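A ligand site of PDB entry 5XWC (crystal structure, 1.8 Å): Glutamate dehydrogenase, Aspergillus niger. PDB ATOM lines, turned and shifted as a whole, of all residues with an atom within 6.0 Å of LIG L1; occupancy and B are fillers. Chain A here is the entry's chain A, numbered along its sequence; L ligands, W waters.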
ATOM      1  N   LYS A  78       7.434 -11.875  18.833  1.00  0.00           N
ATOM      2  CA  LYS A  78       8.426 -12.292  17.867  1.00  0.00           C
ATOM      3  C   LYS A  78       7.888 -11.937  16.481  1.00  0.00           C
ATOM      4  O   LYS A  78       6.734 -12.239  16.160  1.00  0.00           O
ATOM      5  CB  LYS A  78       8.633 -13.803  17.901  1.00  0.00           C
ATOM      6  CG  LYS A  78       9.761 -14.283  17.016  1.00  0.00           C
ATOM      7  CD  LYS A  78      11.101 -14.158  17.681  1.00  0.00           C
ATOM      8  CE  LYS A  78      12.237 -14.362  16.696  1.00  0.00           C
ATOM      9  NZ  LYS A  78      12.510 -13.196  15.807  1.00  0.00           N
ATOM     10  N   GLY A  79       8.744 -11.272  15.714  1.00  0.00           N
ATOM     11  CA  GLY A  79       8.441 -10.999  14.318  1.00  0.00           C
ATOM     12  C   GLY A  79       9.307  -9.886  13.801  1.00  0.00           C
ATOM     13  O   GLY A  79       9.936  -9.162  14.570  1.00  0.00           O
ATOM     14  N   GLY A  80       9.330  -9.741  12.492  1.00  0.00           N
ATOM     15  CA  GLY A  80      10.268  -8.854  11.840  1.00  0.00           C
ATOM     16  C   GLY A  80      10.010  -7.366  11.862  1.00  0.00           C
ATOM     17  O   GLY A  80       8.994  -6.887  12.388  1.00  0.00           O
ATOM     18  N   LEU A  95       0.369  -7.725   9.702  1.00  0.00           N
ATOM     19  CA  LEU A  95       1.534  -8.592   9.813  1.00  0.00           C
ATOM     20  C   LEU A  95       1.693  -9.214  11.207  1.00  0.00           C
ATOM     21  O   LEU A  95       1.921 -10.426  11.354  1.00  0.00           O
ATOM     22  CB  LEU A  95       2.788  -7.810   9.422  1.00  0.00           C
ATOM     23  CG  LEU A  95       2.932  -7.504   7.925  1.00  0.00           C
ATOM     24  CD1 LEU A  95       3.850  -6.322   7.709  1.00  0.00           C
ATOM     25  CD2 LEU A  95       3.394  -8.743   7.158  1.00  0.00           C
ATOM     26  N   GLN A  99       1.310 -13.025  12.385  1.00  0.00           N
ATOM     27  CA  GLN A  99       2.447 -13.592  13.099  1.00  0.00           C
ATOM     28  C   GLN A  99       2.062 -14.417  14.328  1.00  0.00           C
ATOM     29  O   GLN A  99       2.766 -15.386  14.669  1.00  0.00           O
ATOM     30  CB  GLN A  99       3.437 -12.476  13.509  1.00  0.00           C
ATOM     31  CG  GLN A  99       4.840 -12.991  13.759  1.00  0.00           C
ATOM     32  CD  GLN A  99       5.602 -13.259  12.468  1.00  0.00           C
ATOM     33  OE1 GLN A  99       5.538 -12.467  11.548  1.00  0.00           O
ATOM     34  NE2 GLN A  99       6.342 -14.350  12.416  1.00  0.00           N
ATOM     35  N   LYS A 102       0.926 -17.873  12.885  1.00  0.00           N
ATOM     36  CA  LYS A 102       2.097 -18.473  12.272  1.00  0.00           C
ATOM     37  C   LYS A 102       3.026 -19.030  13.332  1.00  0.00           C
ATOM     38  O   LYS A 102       3.489 -20.181  13.264  1.00  0.00           O
ATOM     39  CB  LYS A 102       2.841 -17.441  11.451  1.00  0.00           C
ATOM     40  CG  LYS A 102       4.111 -17.967  10.762  1.00  0.00           C
ATOM     41  CD  LYS A 102       4.944 -16.846  10.134  1.00  0.00           C
ATOM     42  CE  LYS A 102       4.100 -15.815   9.429  1.00  0.00           C
ATOM     43  NZ  LYS A 102       4.936 -14.899   8.633  1.00  0.00           N
ATOM     44  N   ASN A 103       3.319 -18.193  14.327  1.00  0.00           N
ATOM     45  CA  ASN A 103       4.229 -18.637  15.370  1.00  0.00           C
ATOM     46  C   ASN A 103       3.694 -19.822  16.158  1.00  0.00           C
ATOM     47  O   ASN A 103       4.455 -20.731  16.490  1.00  0.00           O
ATOM     48  CB  ASN A 103       4.593 -17.437  16.276  1.00  0.00           C
ATOM     49  CG  ASN A 103       5.432 -16.424  15.539  1.00  0.00           C
ATOM     50  OD1 ASN A 103       5.698 -16.568  14.323  1.00  0.00           O
ATOM     51  ND2 ASN A 103       5.881 -15.397  16.242  1.00  0.00           N
ATOM     52  N   LYS A 114       5.265  -7.299  15.153  1.00  0.00           N
ATOM     53  CA  LYS A 114       5.859  -6.793  13.914  1.00  0.00           C
ATOM     54  C   LYS A 114       6.148  -5.315  14.136  1.00  0.00           C
ATOM     55  O   LYS A 114       5.415  -4.642  14.883  1.00  0.00           O
ATOM     56  CB  LYS A 114       4.900  -6.938  12.724  1.00  0.00           C
ATOM     57  CG  LYS A 114       5.642  -7.088  11.407  1.00  0.00           C
ATOM     58  CD  LYS A 114       6.082  -8.534  11.217  1.00  0.00           C
ATOM     59  CE  LYS A 114       6.863  -8.664   9.922  1.00  0.00           C
ATOM     60  NZ  LYS A 114       6.890 -10.093   9.552  1.00  0.00           N
ATOM     61  N   VAL A 150      11.594  -9.986  20.406  1.00  0.00           N
ATOM     62  CA  VAL A 150      12.767 -10.357  19.621  1.00  0.00           C
ATOM     63  C   VAL A 150      12.454 -10.078  18.131  1.00  0.00           C
ATOM     64  O   VAL A 150      11.827 -10.900  17.487  1.00  0.00           O
ATOM     65  CB  VAL A 150      13.196 -11.819  19.851  1.00  0.00           C
ATOM     66  CG1 VAL A 150      14.408 -12.202  19.010  1.00  0.00           C
ATOM     67  CG2 VAL A 150      13.518 -12.055  21.323  1.00  0.00           C
ATOM     68  N   PRO A 151      12.862  -8.905  17.623  1.00  0.00           N
ATOM     69  CA  PRO A 151      12.655  -8.657  16.200  1.00  0.00           C
ATOM     70  C   PRO A 151      13.673  -9.378  15.284  1.00  0.00           C
ATOM     71  O   PRO A 151      14.451 -10.236  15.710  1.00  0.00           O
ATOM     72  CB  PRO A 151      12.741  -7.145  16.092  1.00  0.00           C
ATOM     73  CG  PRO A 151      12.593  -6.635  17.517  1.00  0.00           C
ATOM     74  CD  PRO A 151      13.299  -7.667  18.291  1.00  0.00           C
ATOM     75  N   ALA A 152      13.574  -9.057  14.000  1.00  0.00           N
ATOM     76  CA  ALA A 152      14.369  -9.675  12.948  1.00  0.00           C
ATOM     77  C   ALA A 152      14.137  -8.822  11.701  1.00  0.00           C
ATOM     78  O   ALA A 152      13.546  -7.729  11.792  1.00  0.00           O
ATOM     79  CB  ALA A 152      13.914 -11.112  12.707  1.00  0.00           C
ATOM     80  N   GLY A 153      14.586  -9.318  10.564  1.00  0.00           N
ATOM     81  CA  GLY A 153      14.347  -8.662   9.285  1.00  0.00           C
ATOM     82  C   GLY A 153      12.964  -8.956   8.736  1.00  0.00           C
ATOM     83  O   GLY A 153      12.175  -9.650   9.370  1.00  0.00           O
ATOM     84  N   ASP A 154      12.713  -8.383   7.568  1.00  0.00           N
ATOM     85  CA  ASP A 154      11.490  -8.489   6.758  1.00  0.00           C
ATOM     86  C   ASP A 154      11.805  -7.625   5.536  1.00  0.00           C
ATOM     87  O   ASP A 154      12.981  -7.443   5.218  1.00  0.00           O
ATOM     88  CB  ASP A 154      10.221  -8.039   7.494  1.00  0.00           C
ATOM     89  CG  ASP A 154       8.918  -8.502   6.809  1.00  0.00           C
ATOM     90  OD1 ASP A 154       8.510  -9.685   6.954  1.00  0.00           O
ATOM     91  OD2 ASP A 154       8.283  -7.644   6.140  1.00  0.00           O
ATOM     92  N   THR A 181      17.023 -11.687  15.824  1.00  0.00           N
ATOM     93  CA  THR A 181      17.480 -12.822  15.045  1.00  0.00           C
ATOM     94  C   THR A 181      17.748 -12.362  13.607  1.00  0.00           C
ATOM     95  O   THR A 181      17.540 -11.176  13.272  1.00  0.00           O
ATOM     96  CB  THR A 181      16.474 -13.989  15.108  1.00  0.00           C
ATOM     97  OG1 THR A 181      15.175 -13.566  14.629  1.00  0.00           O
ATOM     98  CG2 THR A 181      16.364 -14.472  16.519  1.00  0.00           C
ATOM     99  N   ARG A 193      19.501 -19.770   8.842  1.00  0.00           N
ATOM    100  CA  ARG A 193      18.534 -18.661   8.930  1.00  0.00           C
ATOM    101  C   ARG A 193      18.335 -17.888   7.603  1.00  0.00           C
ATOM    102  O   ARG A 193      17.208 -17.576   7.256  1.00  0.00           O
ATOM    103  CB  ARG A 193      18.829 -17.678  10.102  1.00  0.00           C
ATOM    104  CG  ARG A 193      17.757 -16.583  10.248  1.00  0.00           C
ATOM    105  CD  ARG A 193      16.388 -17.165  10.586  1.00  0.00           C
ATOM    106  NE  ARG A 193      15.259 -16.213  10.523  1.00  0.00           N
ATOM    107  CZ  ARG A 193      14.598 -15.836   9.441  1.00  0.00           C
ATOM    108  NH1 ARG A 193      14.985 -16.237   8.210  1.00  0.00           N
ATOM    109  NH2 ARG A 193      13.557 -15.022   9.537  1.00  0.00           N
ATOM    110  N   THR A 197      13.261 -19.291   5.299  1.00  0.00           N
ATOM    111  CA  THR A 197      11.891 -19.025   4.870  1.00  0.00           C
ATOM    112  C   THR A 197      11.626 -19.686   3.503  1.00  0.00           C
ATOM    113  O   THR A 197      10.653 -20.431   3.345  1.00  0.00           O
ATOM    114  CB  THR A 197      11.568 -17.547   4.833  1.00  0.00           C
ATOM    115  OG1 THR A 197      11.812 -16.991   6.151  1.00  0.00           O
ATOM    116  CG2 THR A 197      10.119 -17.350   4.500  1.00  0.00           C
ATOM    117  N   ASN A 346       3.774 -12.593   3.158  1.00  0.00           N
ATOM    118  CA  ASN A 346       2.645 -12.495   4.057  1.00  0.00           C
ATOM    119  C   ASN A 346       1.443 -11.880   3.330  1.00  0.00           C
ATOM    120  O   ASN A 346       1.547 -10.800   2.743  1.00  0.00           O
ATOM    121  CB  ASN A 346       3.023 -11.667   5.293  1.00  0.00           C
ATOM    122  CG  ASN A 346       3.923 -12.452   6.226  1.00  0.00           C
ATOM    123  OD1 ASN A 346       3.535 -13.513   6.687  1.00  0.00           O
ATOM    124  ND2 ASN A 346       5.138 -11.972   6.443  1.00  0.00           N
ATOM    125  N   ASN A 379       5.241 -20.128   5.108  1.00  0.00           N
ATOM    126  CA  ASN A 379       6.400 -19.248   5.295  1.00  0.00           C
ATOM    127  C   ASN A 379       6.940 -19.234   6.750  1.00  0.00           C
ATOM    128  O   ASN A 379       7.910 -18.524   7.015  1.00  0.00           O
ATOM    129  CB  ASN A 379       6.172 -17.857   4.706  1.00  0.00           C
ATOM    130  CG  ASN A 379       5.330 -16.936   5.571  1.00  0.00           C
ATOM    131  OD1 ASN A 379       5.373 -16.996   6.814  1.00  0.00           O
ATOM    132  ND2 ASN A 379       4.549 -16.067   4.911  1.00  0.00           N
ATOM    133  N   ALA A 380       6.407 -20.101   7.597  1.00  0.00           N
ATOM    134  CA  ALA A 380       6.733 -20.196   9.025  1.00  0.00           C
ATOM    135  C   ALA A 380       8.134 -20.685   9.318  1.00  0.00           C
ATOM    136  O   ALA A 380       8.594 -20.628  10.456  1.00  0.00           O
ATOM    137  CB  ALA A 380       5.743 -21.116   9.706  1.00  0.00           C
ATOM    138  N   GLY A 382      10.930 -19.384   8.511  1.00  0.00           N
ATOM    139  CA  GLY A 382      11.844 -18.283   8.842  1.00  0.00           C
ATOM    140  C   GLY A 382      11.803 -18.024  10.335  1.00  0.00           C
ATOM    141  O   GLY A 382      12.825 -18.072  11.023  1.00  0.00           O
ATOM    142  N   VAL A 383      10.606 -17.753  10.824  1.00  0.00           N
ATOM    143  CA  VAL A 383      10.424 -17.487  12.259  1.00  0.00           C
ATOM    144  C   VAL A 383      10.784 -18.727  13.100  1.00  0.00           C
ATOM    145  O   VAL A 383      11.270 -18.609  14.235  1.00  0.00           O
ATOM    146  CB  VAL A 383       9.034 -16.900  12.569  1.00  0.00           C
ATOM    147  CG1 VAL A 383       7.927 -17.946  12.535  1.00  0.00           C
ATOM    148  CG2 VAL A 383       9.062 -16.225  13.973  1.00  0.00           C
ATOM    149  N   ALA A 384      10.527 -19.932  12.566  1.00  0.00           N
ATOM    150  CA  ALA A 384      10.930 -21.159  13.242  1.00  0.00           C
ATOM    151  C   ALA A 384      12.433 -21.195  13.454  1.00  0.00           C
ATOM    152  O   ALA A 384      12.893 -21.447  14.589  1.00  0.00           O
ATOM    153  CB  ALA A 384      10.458 -22.412  12.487  1.00  0.00           C
ATOM    154  N   SER A 386      14.404 -18.582  13.356  1.00  0.00           N
ATOM    155  CA  SER A 386      14.663 -17.518  14.348  1.00  0.00           C
ATOM    156  C   SER A 386      14.514 -18.042  15.783  1.00  0.00           C
ATOM    157  O   SER A 386      15.338 -17.758  16.637  1.00  0.00           O
ATOM    158  CB  SER A 386      13.721 -16.317  14.153  1.00  0.00           C
ATOM    159  OG  SER A 386      14.125 -15.451  13.122  1.00  0.00           O
HETATM  160  O1  LIG L   1       7.113 -12.652   8.376  1.00  0.00           O
HETATM  161  C1  LIG L   1       7.887 -13.432   8.953  1.00  0.00           C
HETATM  162  O2  LIG L   1       7.476 -14.486   9.519  1.00  0.00           O
HETATM  163  C2  LIG L   1       9.311 -13.010   9.043  1.00  0.00           C
HETATM  164  N1  LIG L   1       9.795 -11.874   8.475  1.00  0.00           N
HETATM  165  C3  LIG L   1      10.266 -13.716   9.997  1.00  0.00           C
HETATM  166  C4  LIG L   1      10.334 -12.951  11.288  1.00  0.00           C
HETATM  167  C5  LIG L   1      11.247 -13.532  12.342  1.00  0.00           C
HETATM  168  O3  LIG L   1      11.038 -13.154  13.531  1.00  0.00           O
HETATM  169  O4  LIG L   1      12.164 -14.303  12.013  1.00  0.00           O
HETATM  170  P1  LG2 L   2      13.227  -8.465   0.881  1.00  0.00           P
HETATM  171  O1  LG2 L   2      14.491  -9.274   0.877  1.00  0.00           O
HETATM  172  O2  LG2 L   2      13.224  -7.017   1.113  1.00  0.00           O
HETATM  173  O3  LG2 L   2      12.586  -8.631  -0.603  1.00  0.00           O
HETATM  174  C1  LG2 L   2      11.303  -8.118  -0.897  1.00  0.00           C
HETATM  175  C2  LG2 L   2      11.103  -8.326  -2.413  1.00  0.00           C
HETATM  176  O4  LG2 L   2       9.750  -7.996  -2.701  1.00  0.00           O
HETATM  177  C3  LG2 L   2      11.960  -7.446  -3.293  1.00  0.00           C
HETATM  178  O5  LG2 L   2      12.231  -8.109  -4.562  1.00  0.00           O
HETATM  179  C4  LG2 L   2      11.070  -6.230  -3.448  1.00  0.00           C
HETATM  180  O6  LG2 L   2      11.288  -5.408  -4.593  1.00  0.00           O
HETATM  181  C5  LG2 L   2       9.687  -6.814  -3.501  1.00  0.00           C
HETATM  182  N1  LG2 L   2       8.693  -5.858  -2.966  1.00  0.00           N
HETATM  183  C6  LG2 L   2       8.649  -5.402  -1.678  1.00  0.00           C
HETATM  184  N2  LG2 L   2       7.614  -4.540  -1.510  1.00  0.00           N
HETATM  185  C7  LG2 L   2       7.002  -4.453  -2.693  1.00  0.00           C
HETATM  186  C8  LG2 L   2       5.842  -3.701  -3.178  1.00  0.00           C
HETATM  187  N3  LG2 L   2       5.185  -2.910  -2.311  1.00  0.00           N
HETATM  188  N4  LG2 L   2       5.486  -3.868  -4.475  1.00  0.00           N
HETATM  189  C9  LG2 L   2       6.176  -4.695  -5.296  1.00  0.00           C
HETATM  190  N5  LG2 L   2       7.247  -5.410  -4.912  1.00  0.00           N
HETATM  191  C10 LG2 L   2       7.699  -5.314  -3.638  1.00  0.00           C
HETATM  192  O7  LG2 L   2      12.096  -9.143   1.781  1.00  0.00           O
HETATM  193  P2  LG2 L   2      11.813 -10.682   2.144  1.00  0.00           P
HETATM  194  O8  LG2 L   2      12.242 -11.539   0.988  1.00  0.00           O
HETATM  195  O9  LG2 L   2      12.376 -10.977   3.505  1.00  0.00           O
HETATM  196  O10 LG2 L   2      10.235 -10.632   2.278  1.00  0.00           O
HETATM  197  C11 LG2 L   2       9.346 -11.034   1.204  1.00  0.00           C
HETATM  198  C12 LG2 L   2       7.999 -11.461   1.729  1.00  0.00           C
HETATM  199  O11 LG2 L   2       8.170 -12.605   2.567  1.00  0.00           O
HETATM  200  C13 LG2 L   2       7.280 -10.407   2.601  1.00  0.00           C
HETATM  201  O12 LG2 L   2       5.874 -10.502   2.429  1.00  0.00           O
HETATM  202  C14 LG2 L   2       7.679 -10.813   4.015  1.00  0.00           C
HETATM  203  O13 LG2 L   2       6.844 -10.251   5.052  1.00  0.00           O
HETATM  204  C15 LG2 L   2       7.590 -12.324   3.862  1.00  0.00           C
HETATM  205  N6  LG2 L   2       8.287 -13.140   4.875  1.00  0.00           N
HETATM  206  C16 LG2 L   2       9.583 -12.937   5.132  1.00  0.00           C
HETATM  207  C17 LG2 L   2      10.265 -13.715   6.075  1.00  0.00           C
HETATM  208  C18 LG2 L   2      11.730 -13.578   6.329  1.00  0.00           C
HETATM  209  O14 LG2 L   2      12.264 -14.413   7.081  1.00  0.00           O
HETATM  210  N7  LG2 L   2      12.492 -12.705   5.628  1.00  0.00           N
HETATM  211  C19 LG2 L   2       9.552 -14.726   6.734  1.00  0.00           C
HETATM  212  C20 LG2 L   2       8.214 -14.943   6.414  1.00  0.00           C
HETATM  213  C21 LG2 L   2       7.601 -14.159   5.461  1.00  0.00           C
HETATM  214  P3  LG2 L   2      12.500  -4.341  -4.712  1.00  0.00           P
HETATM  215  O15 LG2 L   2      13.715  -5.306  -4.866  1.00  0.00           O
HETATM  216  O16 LG2 L   2      12.791  -3.598  -3.525  1.00  0.00           O
HETATM  217  O17 LG2 L   2      12.026  -3.487  -5.892  1.00  0.00           O
HETATM  218  O   HOH W   1       8.504 -17.040   9.167  1.00  0.00           O
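OG of Ser 386 lies within hydrogen-bond range of OG1 of Thr 181 (2.6 Å). The side-chain hydroxyl of Thr 181 sits at hydrogen-bond distance from the side-chain amino group of Lys 78, 2.9 Å away. The side-chain amide nitrogen (ND2) of Asn 103 sits at hydrogen-bond distance from the backbone carbonyl oxygen (O) of Lys 78, at 3.3 Å. The side-chain amino group of Lys 102 sits at hydrogen-bond distance from the side-chain amide oxygen of Asn 346, at 2.8 Å. The side-chain amino group of Lys 114 is in salt-bridge range of the side-chain carboxylate of Asp 154, 3.1 Å away. The side-chain amide nitrogen of Asn 379 is in hydrogen-bond range of the side-chain amide oxygen of Asn 346 (3.3 Å). The side-chain amide oxygen of Asn 103 sits at hydrogen-bond distance from the side-chain amide nitrogen of Gln 99 (3.0 Å). N of Gly 382 sits close to OG1 of Thr 197, 3.5 Å away.
CA of Gly 79 touches O3 of LIG L1 (3.5 Å). Gly 80 touches LIG L1. CB of Ala 152 touches C5 of LIG L1, at 3.6 Å. Gly 382 touches LIG L1. CA of Val 383 touches O4 of LIG L1, 3.6 Å away. Hydrophobic or aromatic side chains within 4 Å of LIG L1: Ala 152 and Val 383. The nearest printed residue that does not touch LIG L1 is Thr 181 (4.1 Å).
The side-chain hydroxyl of Ser 386 sits at hydrogen-bond distance from an oxygen (O4) of LIG L1, 2.5 Å away. NZ of Lys 78 lies within salt-bridge range of O3 of LIG L1 (2.7 Å). O2 of LIG L1 lies within salt-bridge range of NZ of Lys 102 (2.7 Å). O1 of LIG L1 is in salt-bridge range of NZ of Lys 114, 2.8 Å away. ND2 of Asn 346 is in hydrogen-bond range of O1 of LIG L1 (2.8 Å). NH2 of Arg 193 is in salt-bridge range of O4 of LIG L1 (2.9 Å). The side-chain carboxylate (OD1) of Asp 154 lies within hydrogen-bond range of a nitrogen (N1) of LIG L1 (3.0 Å). An oxygen (O2) of LIG L1 lies within hydrogen-bond range of the side-chain amide nitrogen of Gln 99 (3.1 Å). N1 of LIG L1 is in hydrogen-bond range of O of Gly 153, at 3.4 Å. N of Asn 346 is in hydrogen-bond range of O12 of LG2 L2 (3.1 Å). The side-chain amide nitrogen (ND2) of Asn 346 lies within hydrogen-bond range of an oxygen (O13) of LG2 L2. NH2 of Arg 193 lies within hydrogen-bond range of O14 of LG2 L2, at 2.8 Å. The side-chain carboxylate of Asp 154 sits at hydrogen-bond distance from an oxygen (O13) of LG2 L2, at 2.6 Å. An oxygen (O14) of LG2 L2 is in hydrogen-bond range of the side-chain hydroxyl (OG1) of Thr 197 (2.8 Å).
Water W1 lies within hydrogen-bond range of O of Asn 379 (2.7 Å), N of Val 383 (2.8 Å), O2 of LIG L1 (2.8 Å) and N of Gly 382 (3.4 Å).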
